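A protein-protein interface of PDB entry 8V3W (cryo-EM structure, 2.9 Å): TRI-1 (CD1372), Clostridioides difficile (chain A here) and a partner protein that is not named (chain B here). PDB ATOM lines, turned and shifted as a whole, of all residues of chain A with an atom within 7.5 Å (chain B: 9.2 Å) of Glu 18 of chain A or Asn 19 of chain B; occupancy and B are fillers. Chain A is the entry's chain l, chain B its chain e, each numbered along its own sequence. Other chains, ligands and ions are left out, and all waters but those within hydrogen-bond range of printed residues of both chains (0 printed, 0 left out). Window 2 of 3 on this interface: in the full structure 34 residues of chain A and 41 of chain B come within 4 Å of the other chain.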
ATOM      1  N   ILE A   4       0.560 -18.418 -27.496  1.00  0.00           N
ATOM      2  CA  ILE A   4       1.726 -17.628 -27.861  1.00  0.00           C
ATOM      3  C   ILE A   4       1.426 -16.655 -28.992  1.00  0.00           C
ATOM      4  O   ILE A   4       2.188 -15.709 -29.210  1.00  0.00           O
ATOM      5  CB  ILE A   4       2.895 -18.555 -28.231  1.00  0.00           C
ATOM      6  CG1 ILE A   4       4.220 -17.805 -28.119  1.00  0.00           C
ATOM      7  CG2 ILE A   4       2.703 -19.123 -29.623  1.00  0.00           C
ATOM      8  CD1 ILE A   4       5.385 -18.564 -28.664  1.00  0.00           C
ATOM      9  N   ASN A  13      11.062 -16.713 -27.865  1.00  0.00           N
ATOM     10  CA  ASN A  13      12.137 -17.512 -27.300  1.00  0.00           C
ATOM     11  C   ASN A  13      11.581 -18.776 -26.645  1.00  0.00           C
ATOM     12  O   ASN A  13      10.405 -18.855 -26.284  1.00  0.00           O
ATOM     13  CB  ASN A  13      12.929 -16.693 -26.287  1.00  0.00           C
ATOM     14  CG  ASN A  13      12.039 -15.969 -25.309  1.00  0.00           C
ATOM     15  OD1 ASN A  13      11.389 -14.985 -25.654  1.00  0.00           O
ATOM     16  ND2 ASN A  13      11.997 -16.456 -24.079  1.00  0.00           N
ATOM     17  N   TYR A  14      12.456 -19.772 -26.482  1.00  0.00           N
ATOM     18  CA  TYR A  14      12.016 -21.091 -26.031  1.00  0.00           C
ATOM     19  C   TYR A  14      11.476 -21.070 -24.603  1.00  0.00           C
ATOM     20  O   TYR A  14      10.588 -21.864 -24.270  1.00  0.00           O
ATOM     21  CB  TYR A  14      13.163 -22.099 -26.157  1.00  0.00           C
ATOM     22  CG  TYR A  14      14.352 -21.814 -25.270  1.00  0.00           C
ATOM     23  CD1 TYR A  14      15.256 -20.809 -25.587  1.00  0.00           C
ATOM     24  CD2 TYR A  14      14.580 -22.558 -24.124  1.00  0.00           C
ATOM     25  CE1 TYR A  14      16.342 -20.546 -24.780  1.00  0.00           C
ATOM     26  CE2 TYR A  14      15.666 -22.302 -23.311  1.00  0.00           C
ATOM     27  CZ  TYR A  14      16.543 -21.297 -23.645  1.00  0.00           C
ATOM     28  OH  TYR A  14      17.626 -21.038 -22.840  1.00  0.00           O
ATOM     29  N   ILE A  15      11.984 -20.176 -23.753  1.00  0.00           N
ATOM     30  CA  ILE A  15      11.497 -20.091 -22.377  1.00  0.00           C
ATOM     31  C   ILE A  15      10.024 -19.698 -22.355  1.00  0.00           C
ATOM     32  O   ILE A  15       9.187 -20.359 -21.720  1.00  0.00           O
ATOM     33  CB  ILE A  15      12.354 -19.094 -21.577  1.00  0.00           C
ATOM     34  CG1 ILE A  15      13.814 -19.548 -21.558  1.00  0.00           C
ATOM     35  CG2 ILE A  15      11.816 -18.935 -20.171  1.00  0.00           C
ATOM     36  CD1 ILE A  15      14.733 -18.613 -20.813  1.00  0.00           C
ATOM     37  N   VAL A  16       9.687 -18.622 -23.066  1.00  0.00           N
ATOM     38  CA  VAL A  16       8.303 -18.166 -23.136  1.00  0.00           C
ATOM     39  C   VAL A  16       7.434 -19.221 -23.804  1.00  0.00           C
ATOM     40  O   VAL A  16       6.277 -19.427 -23.421  1.00  0.00           O
ATOM     41  CB  VAL A  16       8.229 -16.816 -23.869  1.00  0.00           C
ATOM     42  CG1 VAL A  16       6.789 -16.399 -24.080  1.00  0.00           C
ATOM     43  CG2 VAL A  16       8.982 -15.754 -23.094  1.00  0.00           C
ATOM     44  N   GLU A  17       7.982 -19.909 -24.806  1.00  0.00           N
ATOM     45  CA  GLU A  17       7.223 -20.945 -25.498  1.00  0.00           C
ATOM     46  C   GLU A  17       6.829 -22.066 -24.546  1.00  0.00           C
ATOM     47  O   GLU A  17       5.676 -22.510 -24.537  1.00  0.00           O
ATOM     48  CB  GLU A  17       8.038 -21.489 -26.670  1.00  0.00           C
ATOM     49  CG  GLU A  17       8.210 -20.485 -27.789  1.00  0.00           C
ATOM     50  CD  GLU A  17       8.477 -21.131 -29.125  1.00  0.00           C
ATOM     51  OE1 GLU A  17       9.582 -21.680 -29.312  1.00  0.00           O
ATOM     52  OE2 GLU A  17       7.580 -21.089 -29.992  1.00  0.00           O
ATOM     53  N   GLU A  18       7.773 -22.524 -23.720  1.00  0.00           N
ATOM     54  CA  GLU A  18       7.459 -23.572 -22.754  1.00  0.00           C
ATOM     55  C   GLU A  18       6.424 -23.096 -21.742  1.00  0.00           C
ATOM     56  O   GLU A  18       5.455 -23.814 -21.431  1.00  0.00           O
ATOM     57  CB  GLU A  18       8.736 -24.017 -22.045  1.00  0.00           C
ATOM     58  CG  GLU A  18       8.755 -25.482 -21.677  1.00  0.00           C
ATOM     59  CD  GLU A  18       9.409 -26.324 -22.751  1.00  0.00           C
ATOM     60  OE1 GLU A  18       9.772 -25.759 -23.803  1.00  0.00           O
ATOM     61  OE2 GLU A  18       9.557 -27.547 -22.547  1.00  0.00           O
ATOM     62  N   ILE A  19       6.612 -21.878 -21.224  1.00  0.00           N
ATOM     63  CA  ILE A  19       5.698 -21.361 -20.211  1.00  0.00           C
ATOM     64  C   ILE A  19       4.283 -21.262 -20.766  1.00  0.00           C
ATOM     65  O   ILE A  19       3.308 -21.592 -20.083  1.00  0.00           O
ATOM     66  CB  ILE A  19       6.200 -20.009 -19.679  1.00  0.00           C
ATOM     67  CG1 ILE A  19       7.542 -20.190 -18.969  1.00  0.00           C
ATOM     68  CG2 ILE A  19       5.187 -19.396 -18.733  1.00  0.00           C
ATOM     69  CD1 ILE A  19       8.042 -18.946 -18.281  1.00  0.00           C
ATOM     70  N   GLN A  20       4.146 -20.823 -22.018  1.00  0.00           N
ATOM     71  CA  GLN A  20       2.817 -20.692 -22.607  1.00  0.00           C
ATOM     72  C   GLN A  20       2.223 -22.044 -22.982  1.00  0.00           C
ATOM     73  O   GLN A  20       1.000 -22.219 -22.914  1.00  0.00           O
ATOM     74  CB  GLN A  20       2.873 -19.776 -23.827  1.00  0.00           C
ATOM     75  CG  GLN A  20       3.222 -18.334 -23.497  1.00  0.00           C
ATOM     76  CD  GLN A  20       2.281 -17.719 -22.487  1.00  0.00           C
ATOM     77  OE1 GLN A  20       1.080 -17.968 -22.510  1.00  0.00           O
ATOM     78  NE2 GLN A  20       2.825 -16.914 -21.585  1.00  0.00           N
ATOM     79  N   GLY A  21       3.059 -23.007 -23.377  1.00  0.00           N
ATOM     80  CA  GLY A  21       2.540 -24.327 -23.699  1.00  0.00           C
ATOM     81  C   GLY A  21       1.940 -25.030 -22.498  1.00  0.00           C
ATOM     82  O   GLY A  21       0.936 -25.743 -22.618  1.00  0.00           O
ATOM     83  N   ALA A  22       2.549 -24.847 -21.323  1.00  0.00           N
ATOM     84  CA  ALA A  22       1.973 -25.436 -20.114  1.00  0.00           C
ATOM     85  C   ALA A  22       0.535 -24.963 -19.903  1.00  0.00           C
ATOM     86  O   ALA A  22      -0.378 -25.770 -19.662  1.00  0.00           O
ATOM     87  CB  ALA A  22       2.834 -25.096 -18.900  1.00  0.00           C
ATOM     88  N   TYR A  23       0.307 -23.656 -20.019  1.00  0.00           N
ATOM     89  CA  TYR A  23      -1.036 -23.132 -19.818  1.00  0.00           C
ATOM     90  C   TYR A  23      -1.963 -23.502 -20.966  1.00  0.00           C
ATOM     91  O   TYR A  23      -3.176 -23.620 -20.765  1.00  0.00           O
ATOM     92  CB  TYR A  23      -0.979 -21.621 -19.620  1.00  0.00           C
ATOM     93  CG  TYR A  23      -0.501 -21.239 -18.243  1.00  0.00           C
ATOM     94  CD1 TYR A  23      -1.362 -21.271 -17.156  1.00  0.00           C
ATOM     95  CD2 TYR A  23       0.815 -20.866 -18.023  1.00  0.00           C
ATOM     96  CE1 TYR A  23      -0.928 -20.931 -15.892  1.00  0.00           C
ATOM     97  CE2 TYR A  23       1.257 -20.524 -16.764  1.00  0.00           C
ATOM     98  CZ  TYR A  23       0.381 -20.559 -15.704  1.00  0.00           C
ATOM     99  OH  TYR A  23       0.818 -20.218 -14.448  1.00  0.00           O
ATOM    100  N   ASP A  24      -1.416 -23.707 -22.166  1.00  0.00           N
ATOM    101  CA  ASP A  24      -2.217 -24.251 -23.261  1.00  0.00           C
ATOM    102  C   ASP A  24      -2.804 -25.609 -22.889  1.00  0.00           C
ATOM    103  O   ASP A  24      -4.013 -25.844 -23.035  1.00  0.00           O
ATOM    104  CB  ASP A  24      -1.363 -24.370 -24.523  1.00  0.00           C
ATOM    105  CG  ASP A  24      -1.582 -23.225 -25.488  1.00  0.00           C
ATOM    106  OD1 ASP A  24      -2.576 -22.490 -25.326  1.00  0.00           O
ATOM    107  OD2 ASP A  24      -0.758 -23.063 -26.413  1.00  0.00           O
ATOM    108  N   ARG B  13       1.159 -30.452 -11.715  1.00  0.00           N
ATOM    109  CA  ARG B  13       1.145 -30.730 -13.147  1.00  0.00           C
ATOM    110  C   ARG B  13       1.691 -29.554 -13.943  1.00  0.00           C
ATOM    111  O   ARG B  13       2.490 -29.736 -14.870  1.00  0.00           O
ATOM    112  CB  ARG B  13      -0.273 -31.073 -13.599  1.00  0.00           C
ATOM    113  CG  ARG B  13      -0.378 -31.488 -15.053  1.00  0.00           C
ATOM    114  CD  ARG B  13      -1.801 -31.334 -15.563  1.00  0.00           C
ATOM    115  NE  ARG B  13      -2.776 -31.788 -14.580  1.00  0.00           N
ATOM    116  CZ  ARG B  13      -4.000 -31.294 -14.452  1.00  0.00           C
ATOM    117  NH1 ARG B  13      -4.434 -30.318 -15.229  1.00  0.00           N
ATOM    118  NH2 ARG B  13      -4.804 -31.789 -13.518  1.00  0.00           N
ATOM    119  N   THR B  14       1.279 -28.334 -13.589  1.00  0.00           N
ATOM    120  CA  THR B  14       1.794 -27.156 -14.278  1.00  0.00           C
ATOM    121  C   THR B  14       3.295 -27.018 -14.079  1.00  0.00           C
ATOM    122  O   THR B  14       4.026 -26.716 -15.029  1.00  0.00           O
ATOM    123  CB  THR B  14       1.079 -25.900 -13.789  1.00  0.00           C
ATOM    124  OG1 THR B  14       1.148 -25.837 -12.361  1.00  0.00           O
ATOM    125  CG2 THR B  14      -0.369 -25.923 -14.212  1.00  0.00           C
ATOM    126  N   LEU B  15       3.777 -27.241 -12.854  1.00  0.00           N
ATOM    127  CA  LEU B  15       5.212 -27.135 -12.610  1.00  0.00           C
ATOM    128  C   LEU B  15       5.987 -28.180 -13.401  1.00  0.00           C
ATOM    129  O   LEU B  15       7.052 -27.884 -13.955  1.00  0.00           O
ATOM    130  CB  LEU B  15       5.504 -27.264 -11.117  1.00  0.00           C
ATOM    131  CG  LEU B  15       5.329 -25.992 -10.292  1.00  0.00           C
ATOM    132  CD1 LEU B  15       5.834 -26.197  -8.879  1.00  0.00           C
ATOM    133  CD2 LEU B  15       6.051 -24.835 -10.953  1.00  0.00           C
ATOM    134  N   GLU B  16       5.470 -29.408 -13.470  1.00  0.00           N
ATOM    135  CA  GLU B  16       6.180 -30.470 -14.173  1.00  0.00           C
ATOM    136  C   GLU B  16       6.133 -30.281 -15.683  1.00  0.00           C
ATOM    137  O   GLU B  16       7.032 -30.748 -16.390  1.00  0.00           O
ATOM    138  CB  GLU B  16       5.596 -31.831 -13.799  1.00  0.00           C
ATOM    139  CG  GLU B  16       5.860 -32.254 -12.367  1.00  0.00           C
ATOM    140  CD  GLU B  16       5.215 -33.585 -12.029  1.00  0.00           C
ATOM    141  OE1 GLU B  16       4.920 -34.360 -12.965  1.00  0.00           O
ATOM    142  OE2 GLU B  16       4.991 -33.854 -10.831  1.00  0.00           O
ATOM    143  N   ASN B  17       5.098 -29.614 -16.195  1.00  0.00           N
ATOM    144  CA  ASN B  17       4.979 -29.429 -17.637  1.00  0.00           C
ATOM    145  C   ASN B  17       6.035 -28.485 -18.198  1.00  0.00           C
ATOM    146  O   ASN B  17       6.264 -28.485 -19.411  1.00  0.00           O
ATOM    147  CB  ASN B  17       3.587 -28.912 -17.985  1.00  0.00           C
ATOM    148  CG  ASN B  17       2.583 -30.026 -18.150  1.00  0.00           C
ATOM    149  OD1 ASN B  17       2.197 -30.372 -19.266  1.00  0.00           O
ATOM    150  ND2 ASN B  17       2.158 -30.604 -17.035  1.00  0.00           N
ATOM    151  N   ILE B  18       6.674 -27.682 -17.355  1.00  0.00           N
ATOM    152  CA  ILE B  18       7.716 -26.762 -17.796  1.00  0.00           C
ATOM    153  C   ILE B  18       9.042 -27.512 -17.776  1.00  0.00           C
ATOM    154  O   ILE B  18       9.566 -27.836 -16.707  1.00  0.00           O
ATOM    155  CB  ILE B  18       7.768 -25.509 -16.913  1.00  0.00           C
ATOM    156  CG1 ILE B  18       6.394 -24.842 -16.863  1.00  0.00           C
ATOM    157  CG2 ILE B  18       8.817 -24.542 -17.429  1.00  0.00           C
ATOM    158  CD1 ILE B  18       6.368 -23.545 -16.083  1.00  0.00           C
ATOM    159  N   ASN B  19       9.585 -27.792 -18.960  1.00  0.00           N
ATOM    160  CA  ASN B  19      10.853 -28.507 -19.092  1.00  0.00           C
ATOM    161  C   ASN B  19      11.967 -27.482 -19.287  1.00  0.00           C
ATOM    162  O   ASN B  19      12.435 -27.231 -20.396  1.00  0.00           O
ATOM    163  CB  ASN B  19      10.795 -29.502 -20.247  1.00  0.00           C
ATOM    164  CG  ASN B  19       9.577 -30.404 -20.185  1.00  0.00           C
ATOM    165  OD1 ASN B  19       9.156 -30.828 -19.108  1.00  0.00           O
ATOM    166  ND2 ASN B  19       8.996 -30.693 -21.345  1.00  0.00           N
ATOM    167  N   LEU B  20      12.392 -26.880 -18.180  1.00  0.00           N
ATOM    168  CA  LEU B  20      13.445 -25.877 -18.196  1.00  0.00           C
ATOM    169  C   LEU B  20      14.440 -26.157 -17.079  1.00  0.00           C
ATOM    170  O   LEU B  20      14.127 -26.822 -16.090  1.00  0.00           O
ATOM    171  CB  LEU B  20      12.879 -24.459 -18.055  1.00  0.00           C
ATOM    172  CG  LEU B  20      12.216 -23.897 -19.313  1.00  0.00           C
ATOM    173  CD1 LEU B  20      11.800 -22.457 -19.102  1.00  0.00           C
ATOM    174  CD2 LEU B  20      13.146 -24.020 -20.504  1.00  0.00           C
ATOM    175  N   ASP B  21      15.653 -25.632 -17.251  1.00  0.00           N
ATOM    176  CA  ASP B  21      16.729 -25.882 -16.301  1.00  0.00           C
ATOM    177  C   ASP B  21      16.589 -25.090 -15.011  1.00  0.00           C
ATOM    178  O   ASP B  21      17.267 -25.411 -14.031  1.00  0.00           O
ATOM    179  CB  ASP B  21      18.077 -25.564 -16.939  1.00  0.00           C
ATOM    180  CG  ASP B  21      18.550 -26.660 -17.858  1.00  0.00           C
ATOM    181  OD1 ASP B  21      18.772 -27.785 -17.367  1.00  0.00           O
ATOM    182  OD2 ASP B  21      18.694 -26.402 -19.073  1.00  0.00           O
ATOM    183  N   ILE B  22      15.737 -24.065 -14.983  1.00  0.00           N
ATOM    184  CA  ILE B  22      15.585 -23.280 -13.768  1.00  0.00           C
ATOM    185  C   ILE B  22      14.968 -24.118 -12.645  1.00  0.00           C
ATOM    186  O   ILE B  22      14.472 -25.232 -12.854  1.00  0.00           O
ATOM    187  CB  ILE B  22      14.777 -22.000 -14.038  1.00  0.00           C
ATOM    188  CG1 ILE B  22      13.592 -22.246 -14.982  1.00  0.00           C
ATOM    189  CG2 ILE B  22      15.669 -20.937 -14.635  1.00  0.00           C
ATOM    190  CD1 ILE B  22      12.584 -23.268 -14.542  1.00  0.00           C
ATOM    191  N   LYS B  24      12.462 -25.036  -9.418  1.00  0.00           N
ATOM    192  CA  LYS B  24      11.106 -24.907  -8.906  1.00  0.00           C
ATOM    193  C   LYS B  24      11.083 -25.317  -7.439  1.00  0.00           C
ATOM    194  O   LYS B  24      11.486 -26.434  -7.097  1.00  0.00           O
ATOM    195  CB  LYS B  24      10.142 -25.767  -9.722  1.00  0.00           C
ATOM    196  CG  LYS B  24       9.901 -25.244 -11.126  1.00  0.00           C
ATOM    197  CD  LYS B  24      10.796 -25.951 -12.125  1.00  0.00           C
ATOM    198  CE  LYS B  24      10.235 -27.289 -12.559  1.00  0.00           C
ATOM    199  NZ  LYS B  24      10.855 -27.735 -13.833  1.00  0.00           N
ATOM    200  N   LEU B  30       9.248 -18.909 -10.619  1.00  0.00           N
ATOM    201  CA  LEU B  30       8.277 -19.716 -11.343  1.00  0.00           C
ATOM    202  C   LEU B  30       7.240 -20.309 -10.403  1.00  0.00           C
ATOM    203  O   LEU B  30       6.049 -20.335 -10.724  1.00  0.00           O
ATOM    204  CB  LEU B  30       8.999 -20.819 -12.110  1.00  0.00           C
ATOM    205  CG  LEU B  30       8.341 -21.285 -13.403  1.00  0.00           C
ATOM    206  CD1 LEU B  30       8.090 -20.113 -14.332  1.00  0.00           C
ATOM    207  CD2 LEU B  30       9.217 -22.317 -14.073  1.00  0.00           C
ATOM    208  N   MET B  33       4.723 -17.513  -9.302  1.00  0.00           N
ATOM    209  CA  MET B  33       3.827 -17.141 -10.393  1.00  0.00           C
ATOM    210  C   MET B  33       2.822 -18.251 -10.685  1.00  0.00           C
ATOM    211  O   MET B  33       1.622 -17.991 -10.871  1.00  0.00           O
ATOM    212  CB  MET B  33       4.650 -16.798 -11.634  1.00  0.00           C
ATOM    213  CG  MET B  33       3.964 -17.051 -12.957  1.00  0.00           C
ATOM    214  SD  MET B  33       5.152 -17.157 -14.309  1.00  0.00           S
ATOM    215  CE  MET B  33       4.095 -17.670 -15.658  1.00  0.00           C
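The side-chain carboxylate (OE2) of Glu 18 of chain A sits close to the side-chain amide nitrogen (ND2) of Asn 19 of chain B (3.4 Å).
The backbone carbonyl oxygen of Glu 16 of chain B sits close to the side-chain amide oxygen of Asn 19 of chain B.
Among the printed residues, merely in contact across the chains: Ile 15 of chain A with Leu 20 of chain B (3.7 Å), Ile 19 of chain A with Met 33 of chain B (3.7 Å) and Ala 22 of chain A with Asn 17 of chain B (3.996 Å).
Of chain B, only Asn 19 (3.3 Å) comes within 4 Å of Glu 18 of chain A. Of the printed residues of chain B, Ala 22 of chain A touches Asn 17 (3.996 Å). Thr 14 of chain B touches none of the printed residues of chain A. Printed residues of chain A within 4 Å of Asn 19 of chain B: Glu 18. Printed residues of chain A within 4 Å of Leu 20 of chain B: Ile 15.
Of the 13 printed residues of chain A, 4 touch a printed residue of chain B. Printed residues of chain A that touch a printed residue of chain B: Ile 15, Glu 18, Ile 19 and Ala 22. Of the 13 printed residues of chain B, 4 touch a printed residue of chain A. Among the printed residues, 4 pairs touch across the chains. Among the printed residues, no Asp or Glu carboxylate lies within 4 Å of a Lys or Arg side-chain nitrogen of the other chain.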
